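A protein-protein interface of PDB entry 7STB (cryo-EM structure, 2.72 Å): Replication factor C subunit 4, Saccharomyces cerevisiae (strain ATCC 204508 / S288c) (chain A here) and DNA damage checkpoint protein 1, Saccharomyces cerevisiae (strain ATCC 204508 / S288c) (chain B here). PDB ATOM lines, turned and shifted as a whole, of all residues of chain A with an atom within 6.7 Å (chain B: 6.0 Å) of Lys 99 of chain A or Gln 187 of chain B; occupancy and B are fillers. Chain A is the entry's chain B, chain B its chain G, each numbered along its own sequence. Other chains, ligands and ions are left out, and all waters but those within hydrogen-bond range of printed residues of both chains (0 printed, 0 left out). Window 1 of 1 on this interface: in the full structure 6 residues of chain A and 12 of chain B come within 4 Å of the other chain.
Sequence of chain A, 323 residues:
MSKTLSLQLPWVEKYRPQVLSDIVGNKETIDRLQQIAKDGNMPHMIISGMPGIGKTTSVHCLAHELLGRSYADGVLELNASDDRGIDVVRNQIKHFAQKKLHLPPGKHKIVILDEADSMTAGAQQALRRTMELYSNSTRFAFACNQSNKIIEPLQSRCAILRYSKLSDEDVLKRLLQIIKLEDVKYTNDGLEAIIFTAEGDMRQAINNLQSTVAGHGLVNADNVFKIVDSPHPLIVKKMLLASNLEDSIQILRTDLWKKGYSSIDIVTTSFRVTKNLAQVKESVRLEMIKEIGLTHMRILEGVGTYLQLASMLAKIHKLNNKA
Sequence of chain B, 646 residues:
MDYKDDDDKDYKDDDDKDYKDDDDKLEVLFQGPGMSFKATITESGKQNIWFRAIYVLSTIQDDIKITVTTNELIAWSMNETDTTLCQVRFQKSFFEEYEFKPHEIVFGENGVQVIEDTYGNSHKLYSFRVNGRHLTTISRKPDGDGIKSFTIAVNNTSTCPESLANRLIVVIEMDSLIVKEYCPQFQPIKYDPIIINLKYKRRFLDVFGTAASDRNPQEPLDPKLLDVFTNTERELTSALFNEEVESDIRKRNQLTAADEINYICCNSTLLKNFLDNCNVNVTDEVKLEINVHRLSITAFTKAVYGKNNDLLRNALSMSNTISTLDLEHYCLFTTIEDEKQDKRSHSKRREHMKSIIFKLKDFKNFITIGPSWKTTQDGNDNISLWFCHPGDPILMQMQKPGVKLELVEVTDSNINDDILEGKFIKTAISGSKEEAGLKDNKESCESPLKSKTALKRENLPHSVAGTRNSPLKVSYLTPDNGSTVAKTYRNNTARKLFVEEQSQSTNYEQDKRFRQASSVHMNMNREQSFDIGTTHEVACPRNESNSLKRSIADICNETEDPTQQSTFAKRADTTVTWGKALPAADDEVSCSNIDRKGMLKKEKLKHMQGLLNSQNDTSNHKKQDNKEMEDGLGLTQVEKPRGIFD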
ATOM      1  N   ALA A  72      11.865  23.323 -30.832  1.00  0.00           N
ATOM      2  CA  ALA A  72      10.679  22.477 -30.755  1.00  0.00           C
ATOM      3  C   ALA A  72      10.541  21.834 -29.380  1.00  0.00           C
ATOM      4  O   ALA A  72       9.441  21.782 -28.819  1.00  0.00           O
ATOM      5  CB  ALA A  72      10.731  21.405 -31.843  1.00  0.00           C
ATOM      6  N   ASP A  73      11.645  21.339 -28.822  1.00  0.00           N
ATOM      7  CA  ASP A  73      11.612  20.633 -27.549  1.00  0.00           C
ATOM      8  C   ASP A  73      11.784  21.549 -26.343  1.00  0.00           C
ATOM      9  O   ASP A  73      11.628  21.082 -25.210  1.00  0.00           O
ATOM     10  CB  ASP A  73      12.705  19.558 -27.519  1.00  0.00           C
ATOM     11  CG  ASP A  73      12.425  18.416 -28.477  1.00  0.00           C
ATOM     12  OD1 ASP A  73      11.237  18.134 -28.740  1.00  0.00           O
ATOM     13  OD2 ASP A  73      13.394  17.800 -28.967  1.00  0.00           O
ATOM     14  N   GLY A  74      12.091  22.826 -26.551  1.00  0.00           N
ATOM     15  CA  GLY A  74      12.350  23.728 -25.445  1.00  0.00           C
ATOM     16  C   GLY A  74      11.339  24.846 -25.301  1.00  0.00           C
ATOM     17  O   GLY A  74      11.469  25.687 -24.408  1.00  0.00           O
ATOM     18  N   VAL A  75      10.329  24.874 -26.167  1.00  0.00           N
ATOM     19  CA  VAL A  75       9.284  25.890 -26.133  1.00  0.00           C
ATOM     20  C   VAL A  75       7.945  25.192 -25.960  1.00  0.00           C
ATOM     21  O   VAL A  75       7.652  24.215 -26.659  1.00  0.00           O
ATOM     22  CB  VAL A  75       9.284  26.759 -27.404  1.00  0.00           C
ATOM     23  CG1 VAL A  75       8.131  27.757 -27.371  1.00  0.00           C
ATOM     24  CG2 VAL A  75      10.609  27.476 -27.554  1.00  0.00           C
ATOM     25  N   LYS A  94       3.408  21.447 -15.721  1.00  0.00           N
ATOM     26  CA  LYS A  94       4.211  20.769 -14.710  1.00  0.00           C
ATOM     27  C   LYS A  94       5.149  19.747 -15.340  1.00  0.00           C
ATOM     28  O   LYS A  94       6.333  19.683 -14.990  1.00  0.00           O
ATOM     29  CB  LYS A  94       3.298  20.098 -13.684  1.00  0.00           C
ATOM     30  CG  LYS A  94       4.033  19.442 -12.527  1.00  0.00           C
ATOM     31  CD  LYS A  94       3.069  19.011 -11.435  1.00  0.00           C
ATOM     32  CE  LYS A  94       3.785  18.283 -10.307  1.00  0.00           C
ATOM     33  NZ  LYS A  94       4.746  19.164  -9.587  1.00  0.00           N
ATOM     34  N   HIS A  95       4.644  18.940 -16.279  1.00  0.00           N
ATOM     35  CA  HIS A  95       5.488  17.921 -16.895  1.00  0.00           C
ATOM     36  C   HIS A  95       6.538  18.550 -17.801  1.00  0.00           C
ATOM     37  O   HIS A  95       7.671  18.063 -17.873  1.00  0.00           O
ATOM     38  CB  HIS A  95       4.629  16.927 -17.674  1.00  0.00           C
ATOM     39  CG  HIS A  95       3.671  16.161 -16.816  1.00  0.00           C
ATOM     40  ND1 HIS A  95       2.436  15.747 -17.266  1.00  0.00           N
ATOM     41  CD2 HIS A  95       3.763  15.744 -15.531  1.00  0.00           C
ATOM     42  CE1 HIS A  95       1.811  15.103 -16.297  1.00  0.00           C
ATOM     43  NE2 HIS A  95       2.594  15.088 -15.233  1.00  0.00           N
ATOM     44  N   PHE A  96       6.185  19.630 -18.501  1.00  0.00           N
ATOM     45  CA  PHE A  96       7.178  20.320 -19.316  1.00  0.00           C
ATOM     46  C   PHE A  96       8.294  20.887 -18.449  1.00  0.00           C
ATOM     47  O   PHE A  96       9.475  20.776 -18.793  1.00  0.00           O
ATOM     48  CB  PHE A  96       6.514  21.429 -20.130  1.00  0.00           C
ATOM     49  CG  PHE A  96       7.461  22.164 -21.036  1.00  0.00           C
ATOM     50  CD1 PHE A  96       8.111  21.502 -22.064  1.00  0.00           C
ATOM     51  CD2 PHE A  96       7.701  23.517 -20.860  1.00  0.00           C
ATOM     52  CE1 PHE A  96       8.983  22.175 -22.897  1.00  0.00           C
ATOM     53  CE2 PHE A  96       8.572  24.194 -21.692  1.00  0.00           C
ATOM     54  CZ  PHE A  96       9.212  23.522 -22.711  1.00  0.00           C
ATOM     55  N   ALA A  97       7.937  21.494 -17.314  1.00  0.00           N
ATOM     56  CA  ALA A  97       8.948  22.029 -16.411  1.00  0.00           C
ATOM     57  C   ALA A  97       9.812  20.917 -15.832  1.00  0.00           C
ATOM     58  O   ALA A  97      11.031  21.071 -15.702  1.00  0.00           O
ATOM     59  CB  ALA A  97       8.279  22.828 -15.296  1.00  0.00           C
ATOM     60  N   GLN A  98       9.196  19.788 -15.471  1.00  0.00           N
ATOM     61  CA  GLN A  98       9.958  18.661 -14.949  1.00  0.00           C
ATOM     62  C   GLN A  98      10.865  18.036 -16.000  1.00  0.00           C
ATOM     63  O   GLN A  98      11.854  17.391 -15.639  1.00  0.00           O
ATOM     64  CB  GLN A  98       9.013  17.595 -14.394  1.00  0.00           C
ATOM     65  CG  GLN A  98       8.361  17.968 -13.076  1.00  0.00           C
ATOM     66  CD  GLN A  98       7.547  16.832 -12.493  1.00  0.00           C
ATOM     67  OE1 GLN A  98       7.691  15.679 -12.896  1.00  0.00           O
ATOM     68  NE2 GLN A  98       6.684  17.153 -11.538  1.00  0.00           N
ATOM     69  N   LYS A  99      10.553  18.207 -17.282  1.00  0.00           N
ATOM     70  CA  LYS A  99      11.349  17.591 -18.336  1.00  0.00           C
ATOM     71  C   LYS A  99      12.793  18.066 -18.255  1.00  0.00           C
ATOM     72  O   LYS A  99      13.061  19.265 -18.145  1.00  0.00           O
ATOM     73  CB  LYS A  99      10.757  17.928 -19.705  1.00  0.00           C
ATOM     74  CG  LYS A  99      11.340  17.117 -20.852  1.00  0.00           C
ATOM     75  CD  LYS A  99      11.372  17.915 -22.144  1.00  0.00           C
ATOM     76  CE  LYS A  99       9.993  18.436 -22.516  1.00  0.00           C
ATOM     77  NZ  LYS A  99       9.946  18.941 -23.917  1.00  0.00           N
ATOM     78  N   LYS A 100      13.725  17.119 -18.314  1.00  0.00           N
ATOM     79  CA  LYS A 100      15.149  17.413 -18.249  1.00  0.00           C
ATOM     80  C   LYS A 100      15.733  17.369 -19.654  1.00  0.00           C
ATOM     81  O   LYS A 100      15.752  16.309 -20.290  1.00  0.00           O
ATOM     82  CB  LYS A 100      15.872  16.421 -17.338  1.00  0.00           C
ATOM     83  CG  LYS A 100      17.187  16.946 -16.786  1.00  0.00           C
ATOM     84  CD  LYS A 100      18.160  15.818 -16.483  1.00  0.00           C
ATOM     85  CE  LYS A 100      19.525  16.342 -16.061  1.00  0.00           C
ATOM     86  NZ  LYS A 100      20.083  17.338 -17.018  1.00  0.00           N
ATOM     87  N   LEU A 101      16.209  18.514 -20.130  1.00  0.00           N
ATOM     88  CA  LEU A 101      16.832  18.631 -21.436  1.00  0.00           C
ATOM     89  C   LEU A 101      18.350  18.707 -21.275  1.00  0.00           C
ATOM     90  O   LEU A 101      18.892  18.619 -20.171  1.00  0.00           O
ATOM     91  CB  LEU A 101      16.288  19.857 -22.175  1.00  0.00           C
ATOM     92  CG  LEU A 101      15.090  19.620 -23.096  1.00  0.00           C
ATOM     93  CD1 LEU A 101      14.533  20.943 -23.590  1.00  0.00           C
ATOM     94  CD2 LEU A 101      15.466  18.728 -24.268  1.00  0.00           C
ATOM     95  N   LYS A 109      14.758  26.311 -20.733  1.00  0.00           N
ATOM     96  CA  LYS A 109      13.484  26.136 -21.413  1.00  0.00           C
ATOM     97  C   LYS A 109      12.610  27.369 -21.219  1.00  0.00           C
ATOM     98  O   LYS A 109      12.641  28.021 -20.172  1.00  0.00           O
ATOM     99  CB  LYS A 109      12.760  24.896 -20.891  1.00  0.00           C
ATOM    100  CG  LYS A 109      13.603  23.629 -20.896  1.00  0.00           C
ATOM    101  CD  LYS A 109      12.779  22.402 -20.537  1.00  0.00           C
ATOM    102  CE  LYS A 109      12.467  22.345 -19.048  1.00  0.00           C
ATOM    103  NZ  LYS A 109      13.627  21.857 -18.253  1.00  0.00           N
ATOM    104  N   TYR A 134      10.420  25.307 -10.261  1.00  0.00           N
ATOM    105  CA  TYR A 134      11.061  24.934 -11.517  1.00  0.00           C
ATOM    106  C   TYR A 134      11.742  26.116 -12.204  1.00  0.00           C
ATOM    107  O   TYR A 134      11.826  26.158 -13.433  1.00  0.00           O
ATOM    108  CB  TYR A 134      10.042  24.307 -12.468  1.00  0.00           C
ATOM    109  CG  TYR A 134       9.401  23.041 -11.949  1.00  0.00           C
ATOM    110  CD1 TYR A 134      10.132  21.868 -11.834  1.00  0.00           C
ATOM    111  CD2 TYR A 134       8.062  23.017 -11.585  1.00  0.00           C
ATOM    112  CE1 TYR A 134       9.550  20.709 -11.366  1.00  0.00           C
ATOM    113  CE2 TYR A 134       7.471  21.862 -11.115  1.00  0.00           C
ATOM    114  CZ  TYR A 134       8.219  20.711 -11.008  1.00  0.00           C
ATOM    115  OH  TYR A 134       7.636  19.556 -10.539  1.00  0.00           O
ATOM    116  N   SER A 137      15.554  25.668 -14.342  1.00  0.00           N
ATOM    117  CA  SER A 137      15.688  25.215 -15.719  1.00  0.00           C
ATOM    118  C   SER A 137      14.572  25.693 -16.636  1.00  0.00           C
ATOM    119  O   SER A 137      14.678  25.496 -17.851  1.00  0.00           O
ATOM    120  CB  SER A 137      15.746  23.681 -15.775  1.00  0.00           C
ATOM    121  OG  SER A 137      14.505  23.112 -15.396  1.00  0.00           O
ATOM    122  N   THR A 138      13.517  26.304 -16.105  1.00  0.00           N
ATOM    123  CA  THR A 138      12.402  26.797 -16.898  1.00  0.00           C
ATOM    124  C   THR A 138      12.198  28.278 -16.618  1.00  0.00           C
ATOM    125  O   THR A 138      12.280  28.719 -15.468  1.00  0.00           O
ATOM    126  CB  THR A 138      11.111  26.032 -16.586  1.00  0.00           C
ATOM    127  OG1 THR A 138      11.389  24.628 -16.509  1.00  0.00           O
ATOM    128  CG2 THR A 138      10.064  26.283 -17.660  1.00  0.00           C
ATOM    129  N   ASP B  63       4.330  11.059  -8.190  1.00  0.00           N
ATOM    130  CA  ASP B  63       5.477  10.572  -8.943  1.00  0.00           C
ATOM    131  C   ASP B  63       6.096   9.389  -8.211  1.00  0.00           C
ATOM    132  O   ASP B  63       6.402   9.484  -7.018  1.00  0.00           O
ATOM    133  CB  ASP B  63       6.519  11.677  -9.131  1.00  0.00           C
ATOM    134  CG  ASP B  63       6.067  12.751 -10.105  1.00  0.00           C
ATOM    135  OD1 ASP B  63       5.388  12.413 -11.096  1.00  0.00           O
ATOM    136  OD2 ASP B  63       6.395  13.933  -9.879  1.00  0.00           O
ATOM    137  N   TYR B 126      20.895   3.187 -10.660  1.00  0.00           N
ATOM    138  CA  TYR B 126      20.348   4.302 -11.429  1.00  0.00           C
ATOM    139  C   TYR B 126      18.910   4.538 -10.996  1.00  0.00           C
ATOM    140  O   TYR B 126      18.078   3.633 -11.089  1.00  0.00           O
ATOM    141  CB  TYR B 126      20.413   4.026 -12.934  1.00  0.00           C
ATOM    142  CG  TYR B 126      20.022   5.217 -13.777  1.00  0.00           C
ATOM    143  CD1 TYR B 126      20.923   6.242 -14.026  1.00  0.00           C
ATOM    144  CD2 TYR B 126      18.747   5.323 -14.315  1.00  0.00           C
ATOM    145  CE1 TYR B 126      20.569   7.336 -14.791  1.00  0.00           C
ATOM    146  CE2 TYR B 126      18.383   6.412 -15.082  1.00  0.00           C
ATOM    147  CZ  TYR B 126      19.299   7.416 -15.316  1.00  0.00           C
ATOM    148  OH  TYR B 126      18.942   8.503 -16.079  1.00  0.00           O
ATOM    149  N   SER B 127      18.611   5.752 -10.548  1.00  0.00           N
ATOM    150  CA  SER B 127      17.302   6.079 -10.006  1.00  0.00           C
ATOM    151  C   SER B 127      16.677   7.220 -10.791  1.00  0.00           C
ATOM    152  O   SER B 127      17.336   8.222 -11.083  1.00  0.00           O
ATOM    153  CB  SER B 127      17.401   6.460  -8.528  1.00  0.00           C
ATOM    154  OG  SER B 127      17.862   5.368  -7.757  1.00  0.00           O
ATOM    155  N   PHE B 128      15.396   7.072 -11.119  1.00  0.00           N
ATOM    156  CA  PHE B 128      14.666   8.113 -11.825  1.00  0.00           C
ATOM    157  C   PHE B 128      13.265   8.238 -11.242  1.00  0.00           C
ATOM    158  O   PHE B 128      12.811   7.406 -10.452  1.00  0.00           O
ATOM    159  CB  PHE B 128      14.605   7.844 -13.337  1.00  0.00           C
ATOM    160  CG  PHE B 128      14.217   6.439 -13.698  1.00  0.00           C
ATOM    161  CD1 PHE B 128      15.155   5.421 -13.696  1.00  0.00           C
ATOM    162  CD2 PHE B 128      12.916   6.140 -14.060  1.00  0.00           C
ATOM    163  CE1 PHE B 128      14.799   4.131 -14.035  1.00  0.00           C
ATOM    164  CE2 PHE B 128      12.554   4.853 -14.402  1.00  0.00           C
ATOM    165  CZ  PHE B 128      13.497   3.846 -14.390  1.00  0.00           C
ATOM    166  N   ARG B 129      12.595   9.316 -11.634  1.00  0.00           N
ATOM    167  CA  ARG B 129      11.254   9.646 -11.182  1.00  0.00           C
ATOM    168  C   ARG B 129      10.329   9.667 -12.390  1.00  0.00           C
ATOM    169  O   ARG B 129      10.648  10.297 -13.405  1.00  0.00           O
ATOM    170  CB  ARG B 129      11.249  11.003 -10.475  1.00  0.00           C
ATOM    171  CG  ARG B 129       9.896  11.445  -9.963  1.00  0.00           C
ATOM    172  CD  ARG B 129       9.984  12.758  -9.201  1.00  0.00           C
ATOM    173  NE  ARG B 129      10.741  13.771  -9.930  1.00  0.00           N
ATOM    174  CZ  ARG B 129      10.383  15.043 -10.060  1.00  0.00           C
ATOM    175  NH1 ARG B 129       9.277  15.515  -9.507  1.00  0.00           N
ATOM    176  NH2 ARG B 129      11.158  15.865 -10.763  1.00  0.00           N
ATOM    177  N   VAL B 130       9.194   8.979 -12.282  1.00  0.00           N
ATOM    178  CA  VAL B 130       8.248   8.844 -13.383  1.00  0.00           C
ATOM    179  C   VAL B 130       6.845   9.113 -12.861  1.00  0.00           C
ATOM    180  O   VAL B 130       6.484   8.669 -11.767  1.00  0.00           O
ATOM    181  CB  VAL B 130       8.318   7.443 -14.028  1.00  0.00           C
ATOM    182  CG1 VAL B 130       7.502   7.408 -15.309  1.00  0.00           C
ATOM    183  CG2 VAL B 130       9.758   7.052 -14.298  1.00  0.00           C
ATOM    184  N   ASN B 131       6.051   9.831 -13.649  1.00  0.00           N
ATOM    185  CA  ASN B 131       4.658  10.061 -13.289  1.00  0.00           C
ATOM    186  C   ASN B 131       3.954   8.728 -13.058  1.00  0.00           C
ATOM    187  O   ASN B 131       3.903   7.878 -13.952  1.00  0.00           O
ATOM    188  CB  ASN B 131       3.961  10.857 -14.389  1.00  0.00           C
ATOM    189  CG  ASN B 131       2.513  11.155 -14.064  1.00  0.00           C
ATOM    190  OD1 ASN B 131       1.704  10.247 -13.895  1.00  0.00           O
ATOM    191  ND2 ASN B 131       2.181  12.435 -13.972  1.00  0.00           N
ATOM    192  N   ASN B 166      16.340  10.492 -21.855  1.00  0.00           N
ATOM    193  CA  ASN B 166      15.574  10.633 -20.617  1.00  0.00           C
ATOM    194  C   ASN B 166      14.122  10.204 -20.815  1.00  0.00           C
ATOM    195  O   ASN B 166      13.189  10.868 -20.359  1.00  0.00           O
ATOM    196  CB  ASN B 166      15.649  12.067 -20.086  1.00  0.00           C
ATOM    197  CG  ASN B 166      16.968  12.367 -19.404  1.00  0.00           C
ATOM    198  OD1 ASN B 166      17.708  11.458 -19.031  1.00  0.00           O
ATOM    199  ND2 ASN B 166      17.269  13.647 -19.240  1.00  0.00           N
ATOM    200  N   ARG B 167      13.930   9.086 -21.510  1.00  0.00           N
ATOM    201  CA  ARG B 167      12.610   8.521 -21.746  1.00  0.00           C
ATOM    202  C   ARG B 167      12.647   7.024 -21.480  1.00  0.00           C
ATOM    203  O   ARG B 167      13.575   6.331 -21.906  1.00  0.00           O
ATOM    204  CB  ARG B 167      12.138   8.792 -23.178  1.00  0.00           C
ATOM    205  CG  ARG B 167      11.516  10.162 -23.369  1.00  0.00           C
ATOM    206  CD  ARG B 167      11.015  10.353 -24.787  1.00  0.00           C
ATOM    207  NE  ARG B 167      10.831  11.762 -25.117  1.00  0.00           N
ATOM    208  CZ  ARG B 167       9.799  12.495 -24.725  1.00  0.00           C
ATOM    209  NH1 ARG B 167       8.832  11.989 -23.977  1.00  0.00           N
ATOM    210  NH2 ARG B 167       9.736  13.772 -25.091  1.00  0.00           N
ATOM    211  N   GLN B 185       8.391  10.362 -20.017  1.00  0.00           N
ATOM    212  CA  GLN B 185       9.563  11.054 -19.495  1.00  0.00           C
ATOM    213  C   GLN B 185       9.912  10.563 -18.094  1.00  0.00           C
ATOM    214  O   GLN B 185       9.031  10.239 -17.295  1.00  0.00           O
ATOM    215  CB  GLN B 185       9.312  12.561 -19.459  1.00  0.00           C
ATOM    216  CG  GLN B 185       9.097  13.193 -20.819  1.00  0.00           C
ATOM    217  CD  GLN B 185       8.440  14.558 -20.728  1.00  0.00           C
ATOM    218  OE1 GLN B 185       7.979  14.968 -19.663  1.00  0.00           O
ATOM    219  NE2 GLN B 185       8.397  15.268 -21.848  1.00  0.00           N
ATOM    220  N   PHE B 186      11.211  10.514 -17.798  1.00  0.00           N
ATOM    221  CA  PHE B 186      11.686  10.226 -16.453  1.00  0.00           C
ATOM    222  C   PHE B 186      12.808  11.192 -16.100  1.00  0.00           C
ATOM    223  O   PHE B 186      13.650  11.511 -16.943  1.00  0.00           O
ATOM    224  CB  PHE B 186      12.164   8.769 -16.314  1.00  0.00           C
ATOM    225  CG  PHE B 186      13.460   8.468 -17.019  1.00  0.00           C
ATOM    226  CD1 PHE B 186      14.677   8.780 -16.435  1.00  0.00           C
ATOM    227  CD2 PHE B 186      13.461   7.836 -18.248  1.00  0.00           C
ATOM    228  CE1 PHE B 186      15.864   8.492 -17.075  1.00  0.00           C
ATOM    229  CE2 PHE B 186      14.646   7.543 -18.891  1.00  0.00           C
ATOM    230  CZ  PHE B 186      15.849   7.871 -18.304  1.00  0.00           C
ATOM    231  N   GLN B 187      12.812  11.652 -14.848  1.00  0.00           N
ATOM    232  CA  GLN B 187      13.795  12.624 -14.376  1.00  0.00           C
ATOM    233  C   GLN B 187      14.823  11.930 -13.497  1.00  0.00           C
ATOM    234  O   GLN B 187      14.440  11.342 -12.477  1.00  0.00           O
ATOM    235  CB  GLN B 187      13.108  13.746 -13.600  1.00  0.00           C
ATOM    236  CG  GLN B 187      12.286  14.683 -14.468  1.00  0.00           C
ATOM    237  CD  GLN B 187      10.896  14.151 -14.750  1.00  0.00           C
ATOM    238  OE1 GLN B 187      10.361  13.342 -13.993  1.00  0.00           O
ATOM    239  NE2 GLN B 187      10.303  14.600 -15.850  1.00  0.00           N
ATOM    240  N   PRO B 188      16.114  11.943 -13.834  1.00  0.00           N
ATOM    241  CA  PRO B 188      17.101  11.293 -12.963  1.00  0.00           C
ATOM    242  C   PRO B 188      17.122  11.915 -11.575  1.00  0.00           C
ATOM    243  O   PRO B 188      16.919  13.120 -11.407  1.00  0.00           O
ATOM    244  CB  PRO B 188      18.430  11.517 -13.696  1.00  0.00           C
ATOM    245  CG  PRO B 188      18.056  11.811 -15.104  1.00  0.00           C
ATOM    246  CD  PRO B 188      16.735  12.505 -15.044  1.00  0.00           C
ATOM    247  N   ILE B 189      17.368  11.076 -10.569  1.00  0.00           N
ATOM    248  CA  ILE B 189      17.437  11.528  -9.184  1.00  0.00           C
ATOM    249  C   ILE B 189      18.461  10.687  -8.435  1.00  0.00           C
ATOM    250  O   ILE B 189      19.030   9.742  -8.989  1.00  0.00           O
ATOM    251  CB  ILE B 189      16.060  11.452  -8.497  1.00  0.00           C
ATOM    252  CG1 ILE B 189      15.477  10.041  -8.619  1.00  0.00           C
ATOM    253  CG2 ILE B 189      15.107  12.478  -9.093  1.00  0.00           C
ATOM    254  CD1 ILE B 189      14.348   9.766  -7.655  1.00  0.00           C
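Lys 99 of chain A touches two residues of chain B.
Gln 187 of chain B touches just these residues of chain A: Gln 98 and Lys 99.
Printed residues of chain A within 4 Å of Arg 129 of chain B: Gln 98 (3.7 Å).
Printed residues of chain A within 4 Å of Asn 131 of chain B: His 95 (3.0 Å).
Of the printed residues of chain B, Lys 100 of chain A touches Asn 166 (3.2 Å) and Pro 188 (3.9 Å).
The nearest residue of chain B that does not touch Lys 99 of chain A is Arg 167 of chain B (5.3 Å).
The nearest printed residue of chain A that does not touch Gln 187 of chain B is Lys 100 of chain A (4.8 Å).
The nearest printed residue of chain B that does not touch Lys 100 of chain A is Gln 187 of chain B (4.8 Å).
O of His 95 of chain A touches OE1 of Gln 185 of chain B, at 3.6 Å.
Gln 98 of chain A touches Asp 63 of chain B (NE2 to OD2, 3.6 Å).
Gln 98 of chain A touches Arg 129 of chain B.
Lys 99 of chain A touches Gln 185 of chain B.
Lys 99 of chain A touches Gln 187 of chain B (N to NE2, 3.9 Å).
Lys 100 of chain A touches Pro 188 of chain B (CD to CD, 3.9 Å).
ND2 of Asn 131 of chain B sits at hydrogen-bond distance from NE2 of His 95 of chain A (3.0 Å).
The backbone carbonyl oxygen of Gln 98 of chain A sits close to the side-chain amide nitrogen of Gln 187 of chain B.
The backbone carbonyl oxygen (O) of Lys 100 of chain A lies within hydrogen-bond range of the side-chain amide nitrogen (ND2) of Asn 166 of chain B (3.2 Å).
Printed residues of chain A that touch a printed residue of chain B: His 95, Gln 98, Lys 99 and Lys 100.
Hydrophobic or aromatic side chains of chain B within 4 Å of the printed part of chain A: Pro 188.
Among the printed residues, no Asp or Glu carboxylate lies within 4 Å of a Lys or Arg side-chain nitrogen of the other chain.
The backbone carbonyl oxygen of Asp 73 of chain A is in hydrogen-bond range of the side-chain amino group of Lys 99 of chain A (3.0 Å).
The side-chain amide nitrogen (NE2) of Gln 98 of chain A sits close to the side-chain amino group (NZ) of Lys 94 of chain A (3.4 Å).
The side-chain hydroxyl (OH) of Tyr 134 of chain A sits at hydrogen-bond distance from the side-chain amide nitrogen (NE2) of Gln 98 of chain A (2.8 Å).
O of Lys 99 of chain A is in hydrogen-bond range of NZ of Lys 109 of chain A (2.7 Å).
The guanidinium group (NH1) of Arg 129 of chain B lies within salt-bridge range of the side-chain carboxylate (OD2) of Asp 63 of chain B (3.3 Å).
O of Gln 187 of chain B sits at hydrogen-bond distance from N of Arg 129 of chain B (2.9 Å).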
